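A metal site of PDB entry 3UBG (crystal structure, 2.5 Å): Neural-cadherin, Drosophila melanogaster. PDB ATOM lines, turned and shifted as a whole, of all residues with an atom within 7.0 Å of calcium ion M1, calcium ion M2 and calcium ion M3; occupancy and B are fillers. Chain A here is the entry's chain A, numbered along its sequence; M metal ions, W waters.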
ATOM      1  N   GLU A  13      -7.443  17.654  14.320  1.00  0.00           N
ATOM      2  CA  GLU A  13      -7.087  18.571  15.405  1.00  0.00           C
ATOM      3  C   GLU A  13      -8.260  18.738  16.377  1.00  0.00           C
ATOM      4  O   GLU A  13      -8.070  19.022  17.569  1.00  0.00           O
ATOM      5  CB  GLU A  13      -6.637  19.919  14.858  1.00  0.00           C
ATOM      6  CG  GLU A  13      -7.723  20.675  14.119  1.00  0.00           C
ATOM      7  CD  GLU A  13      -7.235  21.955  13.454  1.00  0.00           C
ATOM      8  OE1 GLU A  13      -7.715  22.245  12.349  1.00  0.00           O
ATOM      9  OE2 GLU A  13      -6.368  22.665  14.022  1.00  0.00           O
ATOM     10  N   TRP A  58      -5.105  20.675  20.539  1.00  0.00           N
ATOM     11  CA  TRP A  58      -4.451  20.450  19.281  1.00  0.00           C
ATOM     12  C   TRP A  58      -4.786  21.559  18.302  1.00  0.00           C
ATOM     13  O   TRP A  58      -5.905  22.085  18.311  1.00  0.00           O
ATOM     14  CB  TRP A  58      -4.823  19.070  18.749  1.00  0.00           C
ATOM     15  CG  TRP A  58      -4.161  17.951  19.533  1.00  0.00           C
ATOM     16  CD1 TRP A  58      -3.275  18.089  20.567  1.00  0.00           C
ATOM     17  CD2 TRP A  58      -4.361  16.551  19.361  1.00  0.00           C
ATOM     18  NE1 TRP A  58      -2.887  16.855  21.029  1.00  0.00           N
ATOM     19  CE2 TRP A  58      -3.540  15.890  20.307  1.00  0.00           C
ATOM     20  CE3 TRP A  58      -5.139  15.787  18.483  1.00  0.00           C
ATOM     21  CZ2 TRP A  58      -3.479  14.490  20.395  1.00  0.00           C
ATOM     22  CZ3 TRP A  58      -5.078  14.381  18.578  1.00  0.00           C
ATOM     23  CH2 TRP A  58      -4.248  13.753  19.525  1.00  0.00           C
ATOM     24  N   ASP A  59      -3.812  21.924  17.471  1.00  0.00           N
ATOM     25  CA  ASP A  59      -3.966  23.022  16.542  1.00  0.00           C
ATOM     26  C   ASP A  59      -3.093  22.788  15.309  1.00  0.00           C
ATOM     27  O   ASP A  59      -1.873  22.981  15.338  1.00  0.00           O
ATOM     28  CB  ASP A  59      -3.654  24.362  17.222  1.00  0.00           C
ATOM     29  CG  ASP A  59      -3.796  25.570  16.290  1.00  0.00           C
ATOM     30  OD1 ASP A  59      -4.370  25.454  15.189  1.00  0.00           O
ATOM     31  OD2 ASP A  59      -3.316  26.644  16.682  1.00  0.00           O
ATOM     32  N   TYR A  60      -3.757  22.349  14.238  1.00  0.00           N
ATOM     33  CA  TYR A  60      -3.139  22.056  12.966  1.00  0.00           C
ATOM     34  C   TYR A  60      -2.370  23.274  12.423  1.00  0.00           C
ATOM     35  O   TYR A  60      -1.297  23.133  11.841  1.00  0.00           O
ATOM     36  CB  TYR A  60      -4.235  21.625  11.989  1.00  0.00           C
ATOM     37  CG  TYR A  60      -3.735  21.263  10.603  1.00  0.00           C
ATOM     38  CD1 TYR A  60      -3.401  19.960  10.264  1.00  0.00           C
ATOM     39  CD2 TYR A  60      -3.616  22.249   9.618  1.00  0.00           C
ATOM     40  CE1 TYR A  60      -2.948  19.638   8.987  1.00  0.00           C
ATOM     41  CE2 TYR A  60      -3.167  21.945   8.368  1.00  0.00           C
ATOM     42  CZ  TYR A  60      -2.820  20.651   8.048  1.00  0.00           C
ATOM     43  OH  TYR A  60      -2.376  20.385   6.764  1.00  0.00           O
ATOM     44  N   GLU A  61      -2.906  24.475  12.638  1.00  0.00           N
ATOM     45  CA  GLU A  61      -2.228  25.696  12.252  1.00  0.00           C
ATOM     46  C   GLU A  61      -0.888  25.931  12.969  1.00  0.00           C
ATOM     47  O   GLU A  61       0.021  26.500  12.385  1.00  0.00           O
ATOM     48  CB  GLU A  61      -3.154  26.915  12.402  1.00  0.00           C
ATOM     49  CG  GLU A  61      -4.223  27.010  11.325  1.00  0.00           C
ATOM     50  CD  GLU A  61      -5.191  25.828  11.306  1.00  0.00           C
ATOM     51  OE1 GLU A  61      -5.630  25.393  12.399  1.00  0.00           O
ATOM     52  OE2 GLU A  61      -5.515  25.315  10.205  1.00  0.00           O
ATOM     53  N   GLU A  62      -0.735  25.503  14.203  1.00  0.00           N
ATOM     54  CA  GLU A  62       0.555  25.692  14.848  1.00  0.00           C
ATOM     55  C   GLU A  62       1.591  24.577  14.636  1.00  0.00           C
ATOM     56  O   GLU A  62       2.750  24.744  14.989  1.00  0.00           O
ATOM     57  CB  GLU A  62       0.401  25.999  16.346  1.00  0.00           C
ATOM     58  CG  GLU A  62      -0.273  27.342  16.649  1.00  0.00           C
ATOM     59  CD  GLU A  62       0.172  28.453  15.715  1.00  0.00           C
ATOM     60  OE1 GLU A  62       1.396  28.584  15.467  1.00  0.00           O
ATOM     61  OE2 GLU A  62      -0.709  29.194  15.212  1.00  0.00           O
ATOM     62  N   LYS A  97      -4.995  16.142  11.429  1.00  0.00           N
ATOM     63  CA  LYS A  97      -5.759  16.518  10.259  1.00  0.00           C
ATOM     64  C   LYS A  97      -6.467  17.847  10.464  1.00  0.00           C
ATOM     65  O   LYS A  97      -6.995  18.114  11.535  1.00  0.00           O
ATOM     66  CB  LYS A  97      -6.760  15.415   9.935  1.00  0.00           C
ATOM     67  CG  LYS A  97      -6.094  14.217   9.301  1.00  0.00           C
ATOM     68  CD  LYS A  97      -7.095  13.167   8.980  1.00  0.00           C
ATOM     69  CE  LYS A  97      -7.435  12.389  10.208  1.00  0.00           C
ATOM     70  NZ  LYS A  97      -8.486  11.399   9.935  1.00  0.00           N
ATOM     71  N   ASP A  98      -6.459  18.672   9.433  1.00  0.00           N
ATOM     72  CA  ASP A  98      -7.021  20.001   9.519  1.00  0.00           C
ATOM     73  C   ASP A  98      -8.546  19.969   9.548  1.00  0.00           C
ATOM     74  O   ASP A  98      -9.170  19.235   8.791  1.00  0.00           O
ATOM     75  CB  ASP A  98      -6.583  20.844   8.325  1.00  0.00           C
ATOM     76  CG  ASP A  98      -7.156  22.236   8.360  1.00  0.00           C
ATOM     77  OD1 ASP A  98      -7.043  22.858   9.424  1.00  0.00           O
ATOM     78  OD2 ASP A  98      -7.734  22.699   7.354  1.00  0.00           O
ATOM     79  N   VAL A  99      -9.128  20.790  10.418  1.00  0.00           N
ATOM     80  CA  VAL A  99     -10.552  21.018  10.469  1.00  0.00           C
ATOM     81  C   VAL A  99     -10.750  22.526  10.280  1.00  0.00           C
ATOM     82  O   VAL A  99      -9.871  23.315  10.579  1.00  0.00           O
ATOM     83  CB  VAL A  99     -11.147  20.505  11.823  1.00  0.00           C
ATOM     84  CG1 VAL A  99     -12.526  21.052  12.045  1.00  0.00           C
ATOM     85  CG2 VAL A  99     -11.188  18.971  11.872  1.00  0.00           C
ATOM     86  N   ASN A 100     -11.882  22.945   9.749  1.00  0.00           N
ATOM     87  CA  ASN A 100     -12.071  24.368   9.531  1.00  0.00           C
ATOM     88  C   ASN A 100     -12.501  25.029  10.831  1.00  0.00           C
ATOM     89  O   ASN A 100     -13.664  24.952  11.221  1.00  0.00           O
ATOM     90  CB  ASN A 100     -13.101  24.608   8.428  1.00  0.00           C
ATOM     91  CG  ASN A 100     -13.041  26.020   7.865  1.00  0.00           C
ATOM     92  OD1 ASN A 100     -12.907  26.988   8.602  1.00  0.00           O
ATOM     93  ND2 ASN A 100     -13.184  26.143   6.557  1.00  0.00           N
ATOM     94  N   ASP A 101     -11.560  25.677  11.500  1.00  0.00           N
ATOM     95  CA  ASP A 101     -11.775  26.086  12.876  1.00  0.00           C
ATOM     96  C   ASP A 101     -11.079  27.398  13.233  1.00  0.00           C
ATOM     97  O   ASP A 101     -10.980  27.754  14.407  1.00  0.00           O
ATOM     98  CB  ASP A 101     -11.320  24.977  13.826  1.00  0.00           C
ATOM     99  CG  ASP A 101      -9.814  24.857  13.920  1.00  0.00           C
ATOM    100  OD1 ASP A 101      -9.116  25.313  12.988  1.00  0.00           O
ATOM    101  OD2 ASP A 101      -9.306  24.300  14.917  1.00  0.00           O
ATOM    102  N   GLU A 102     -10.573  28.101  12.232  1.00  0.00           N
ATOM    103  CA  GLU A 102      -9.951  29.404  12.469  1.00  0.00           C
ATOM    104  C   GLU A 102     -10.675  30.514  11.718  1.00  0.00           C
ATOM    105  O   GLU A 102     -11.040  30.364  10.559  1.00  0.00           O
ATOM    106  CB  GLU A 102      -8.468  29.375  12.090  1.00  0.00           C
ATOM    107  CG  GLU A 102      -7.683  28.280  12.801  1.00  0.00           C
ATOM    108  CD  GLU A 102      -7.727  28.417  14.315  1.00  0.00           C
ATOM    109  OE1 GLU A 102      -8.167  29.469  14.829  1.00  0.00           O
ATOM    110  OE2 GLU A 102      -7.307  27.487  15.012  1.00  0.00           O
ATOM    111  N   PRO A 103     -10.920  31.645  12.377  1.00  0.00           N
ATOM    112  CA  PRO A 103     -11.650  32.720  11.700  1.00  0.00           C
ATOM    113  C   PRO A 103     -10.810  33.404  10.612  1.00  0.00           C
ATOM    114  O   PRO A 103      -9.578  33.391  10.695  1.00  0.00           O
ATOM    115  CB  PRO A 103     -11.961  33.694  12.846  1.00  0.00           C
ATOM    116  CG  PRO A 103     -10.852  33.471  13.847  1.00  0.00           C
ATOM    117  CD  PRO A 103     -10.552  31.988  13.762  1.00  0.00           C
ATOM    118  N   PRO A 104     -11.466  33.988   9.589  1.00  0.00           N
ATOM    119  CA  PRO A 104     -10.765  34.807   8.598  1.00  0.00           C
ATOM    120  C   PRO A 104     -10.343  36.175   9.132  1.00  0.00           C
ATOM    121  O   PRO A 104     -10.857  36.643  10.143  1.00  0.00           O
ATOM    122  CB  PRO A 104     -11.816  35.005   7.513  1.00  0.00           C
ATOM    123  CG  PRO A 104     -13.112  34.944   8.261  1.00  0.00           C
ATOM    124  CD  PRO A 104     -12.898  33.860   9.274  1.00  0.00           C
ATOM    125  N   ASP A 134      -7.865  33.317   5.268  1.00  0.00           N
ATOM    126  CA  ASP A 134      -8.337  32.403   6.293  1.00  0.00           C
ATOM    127  C   ASP A 134      -7.330  31.260   6.415  1.00  0.00           C
ATOM    128  O   ASP A 134      -6.865  30.739   5.414  1.00  0.00           O
ATOM    129  CB  ASP A 134      -9.712  31.873   5.918  1.00  0.00           C
ATOM    130  CG  ASP A 134     -10.273  30.946   6.960  1.00  0.00           C
ATOM    131  OD1 ASP A 134      -9.744  29.811   7.140  1.00  0.00           O
ATOM    132  OD2 ASP A 134     -11.254  31.372   7.597  1.00  0.00           O
ATOM    133  N   PRO A 135      -6.989  30.867   7.646  1.00  0.00           N
ATOM    134  CA  PRO A 135      -5.896  29.944   7.938  1.00  0.00           C
ATOM    135  C   PRO A 135      -6.171  28.500   7.544  1.00  0.00           C
ATOM    136  O   PRO A 135      -5.232  27.762   7.337  1.00  0.00           O
ATOM    137  CB  PRO A 135      -5.730  30.050   9.461  1.00  0.00           C
ATOM    138  CG  PRO A 135      -6.460  31.298   9.856  1.00  0.00           C
ATOM    139  CD  PRO A 135      -7.576  31.439   8.881  1.00  0.00           C
ATOM    140  N   ASP A 136      -7.422  28.096   7.415  1.00  0.00           N
ATOM    141  CA  ASP A 136      -7.699  26.693   7.129  1.00  0.00           C
ATOM    142  C   ASP A 136      -7.392  26.334   5.675  1.00  0.00           C
ATOM    143  O   ASP A 136      -7.301  27.212   4.822  1.00  0.00           O
ATOM    144  CB  ASP A 136      -9.137  26.359   7.516  1.00  0.00           C
ATOM    145  CG  ASP A 136      -9.422  26.719   8.970  1.00  0.00           C
ATOM    146  OD1 ASP A 136      -8.571  26.493   9.823  1.00  0.00           O
ATOM    147  OD2 ASP A 136     -10.482  27.272   9.278  1.00  0.00           O
ATOM    148  N   THR A 137      -7.196  25.048   5.403  1.00  0.00           N
ATOM    149  CA  THR A 137      -6.931  24.590   4.039  1.00  0.00           C
ATOM    150  C   THR A 137      -8.226  24.613   3.230  1.00  0.00           C
ATOM    151  O   THR A 137      -8.195  24.547   2.011  1.00  0.00           O
ATOM    152  CB  THR A 137      -6.362  23.145   4.014  1.00  0.00           C
ATOM    153  OG1 THR A 137      -7.364  22.203   4.436  1.00  0.00           O
ATOM    154  CG2 THR A 137      -5.149  23.004   4.923  1.00  0.00           C
ATOM    155  N   ASP A 138      -9.346  24.765   3.923  1.00  0.00           N
ATOM    156  CA  ASP A 138     -10.677  24.477   3.405  1.00  0.00           C
ATOM    157  C   ASP A 138     -11.615  25.707   3.425  1.00  0.00           C
ATOM    158  O   ASP A 138     -12.831  25.575   3.608  1.00  0.00           O
ATOM    159  CB  ASP A 138     -11.244  23.357   4.272  1.00  0.00           C
ATOM    160  CG  ASP A 138     -12.634  22.927   3.849  1.00  0.00           C
ATOM    161  OD1 ASP A 138     -13.003  23.106   2.667  1.00  0.00           O
ATOM    162  OD2 ASP A 138     -13.354  22.371   4.728  1.00  0.00           O
ATOM    163  N   HIS A 139     -11.067  26.893   3.230  1.00  0.00           N
ATOM    164  CA  HIS A 139     -11.860  28.126   3.362  1.00  0.00           C
ATOM    165  C   HIS A 139     -12.763  28.442   2.175  1.00  0.00           C
ATOM    166  O   HIS A 139     -12.600  27.934   1.078  1.00  0.00           O
ATOM    167  CB  HIS A 139     -10.920  29.300   3.566  1.00  0.00           C
ATOM    168  CG  HIS A 139      -9.881  29.414   2.511  1.00  0.00           C
ATOM    169  ND1 HIS A 139     -10.143  29.924   1.268  1.00  0.00           N
ATOM    170  CD2 HIS A 139      -8.576  29.055   2.514  1.00  0.00           C
ATOM    171  CE1 HIS A 139      -9.038  29.890   0.540  1.00  0.00           C
ATOM    172  NE2 HIS A 139      -8.070  29.374   1.278  1.00  0.00           N
ATOM    173  N   ASN A 140     -13.733  29.313   2.423  1.00  0.00           N
ATOM    174  CA  ASN A 140     -14.700  29.738   1.424  1.00  0.00           C
ATOM    175  C   ASN A 140     -15.209  31.127   1.783  1.00  0.00           C
ATOM    176  O   ASN A 140     -16.245  31.263   2.437  1.00  0.00           O
ATOM    177  CB  ASN A 140     -15.854  28.735   1.372  1.00  0.00           C
ATOM    178  CG  ASN A 140     -16.942  29.126   0.374  1.00  0.00           C
ATOM    179  OD1 ASN A 140     -16.673  29.747  -0.658  1.00  0.00           O
ATOM    180  ND2 ASN A 140     -18.180  28.741   0.679  1.00  0.00           N
ATOM    181  N   ASP A 185     -15.992  33.004   6.562  1.00  0.00           N
ATOM    182  CA  ASP A 185     -15.619  31.744   5.951  1.00  0.00           C
ATOM    183  C   ASP A 185     -16.866  30.876   6.032  1.00  0.00           C
ATOM    184  O   ASP A 185     -17.225  30.391   7.109  1.00  0.00           O
ATOM    185  CB  ASP A 185     -14.422  31.098   6.658  1.00  0.00           C
ATOM    186  CG  ASP A 185     -14.105  29.701   6.120  1.00  0.00           C
ATOM    187  OD1 ASP A 185     -14.720  29.285   5.115  1.00  0.00           O
ATOM    188  OD2 ASP A 185     -13.215  29.029   6.688  1.00  0.00           O
ATOM    189  N   ASN A 187     -17.329  28.036   5.075  1.00  0.00           N
ATOM    190  CA  ASN A 187     -17.046  26.630   5.329  1.00  0.00           C
ATOM    191  C   ASN A 187     -16.835  26.302   6.805  1.00  0.00           C
ATOM    192  O   ASN A 187     -16.504  25.168   7.130  1.00  0.00           O
ATOM    193  CB  ASN A 187     -15.821  26.173   4.547  1.00  0.00           C
ATOM    194  CG  ASN A 187     -16.165  25.753   3.152  1.00  0.00           C
ATOM    195  OD1 ASN A 187     -17.311  25.887   2.717  1.00  0.00           O
ATOM    196  ND2 ASN A 187     -15.172  25.253   2.420  1.00  0.00           N
ATOM    197  N   GLY A 188     -17.017  27.288   7.679  1.00  0.00           N
ATOM    198  CA  GLY A 188     -16.768  27.094   9.106  1.00  0.00           C
ATOM    199  C   GLY A 188     -17.880  27.646   9.984  1.00  0.00           C
ATOM    200  O   GLY A 188     -17.974  28.865  10.187  1.00  0.00           O
ATOM    201  N   GLN A 196     -17.786  31.636  10.958  1.00  0.00           N
ATOM    202  CA  GLN A 196     -16.587  32.359  11.362  1.00  0.00           C
ATOM    203  C   GLN A 196     -16.441  33.693  10.609  1.00  0.00           C
ATOM    204  O   GLN A 196     -16.683  33.768   9.407  1.00  0.00           O
ATOM    205  CB  GLN A 196     -15.335  31.535  11.117  1.00  0.00           C
ATOM    206  CG  GLN A 196     -15.327  30.164  11.736  1.00  0.00           C
ATOM    207  CD  GLN A 196     -14.465  29.223  10.916  1.00  0.00           C
ATOM    208  OE1 GLN A 196     -14.065  29.549   9.803  1.00  0.00           O
ATOM    209  NE2 GLN A 196     -14.188  28.046  11.450  1.00  0.00           N
HETATM  210 CA    CA M   1      -7.798  24.422  11.017  1.00  0.00          CA
HETATM  211 CA    CA M   2     -11.753  29.195   8.628  1.00  0.00          CA
HETATM  212 CA    CA M   3      -6.811  25.095  14.594  1.00  0.00          CA
HETATM  213  O   HOH W   1      -6.906  24.498  17.276  1.00  0.00           O
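OD2 of Asp 98 lies within hydrogen-bond range of OG1 of Thr 137 (3.0 Å). The side-chain carboxylate (OD1) of Asp 185 lies within hydrogen-bond range of the backbone NH (N) of Asn 187. The side-chain carboxylate (OD1) of Asp 185 is in hydrogen-bond range of the backbone NH (N) of Asn 140, 2.9 Å away. The backbone carbonyl oxygen (O) of Asp 138 lies within hydrogen-bond range of the side-chain amide nitrogen (ND2) of Asn 100, at 3.0 Å. N of Tyr 60 lies close to OE2 of Glu 13, at 2.6 Å. The backbone NH (N) of Glu 13 lies within hydrogen-bond range of the backbone carbonyl oxygen (O) of Lys 97 (2.9 Å). The backbone NH (N) of Gln 196 is in hydrogen-bond range of the backbone carbonyl oxygen (O) of Gly 188.
Within 4 Å of calcium ion M1: Glu 13, Glu 61, Asp 98, Val 99, Asp 101 and Asp 136.
Of the 25 residues printed, 6 come within 4 Å of calcium ion M2. The nearest printed residue that does not touch calcium ion M2 is Asp 101 (4.5 Å).
Within 4 Å of calcium ion M3: Glu 13, Asp 59, Glu 61, Asp 101 and Glu 102. The nearest printed residue that does not touch calcium ion M3 is Tyr 60 (4.1 Å).
Calcium ion M1 is bound by OD1 of Asp 98 (2.4 Å). O of Val 99 is bound to calcium ion M1, 2.4 Å away. Calcium ion M1 is bound by the side-chain carboxylate (OD1) of Asp 136. OD1 of Asp 101 binds calcium ion M1, at 2.5 Å. Calcium ion M1 is bound by OE1 of Glu 13 (2.6 Å). OE2 of Glu 61 is bound to calcium ion M1, at 2.6 Å. The side-chain carboxylate (OE1) of Glu 61 binds calcium ion M1 (2.7 Å).
Calcium ion M2 is bound by O of Glu 102. Calcium ion M2 is bound by the side-chain carboxylate (OD2) of Asp 136. Calcium ion M2 is bound by OD2 of Asp 185. OD2 of Asp 134 is bound to calcium ion M2, at 2.5 Å. OD1 of Asn 100 binds calcium ion M2 (2.5 Å). OD1 of Asp 134 binds calcium ion M2 (2.6 Å). Calcium ion M2 is bound by OE1 of Gln 196 (2.6 Å).
The side-chain carboxylate (OE2) of Glu 102 is bound to calcium ion M3 (2.5 Å). Calcium ion M3 is bound by OE1 of Glu 61. The side-chain carboxylate (OE2) of Glu 13 is bound to calcium ion M3 (2.5 Å). Calcium ion M3 is bound by OD1 of Asp 59 (2.5 Å). Calcium ion M3 is bound by the side-chain carboxylate (OD2) of Asp 101, at 2.6 Å. Calcium ion M3 is bound by water W1 (2.7 Å). OD1 of Asp 101 is bound to calcium ion M3.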
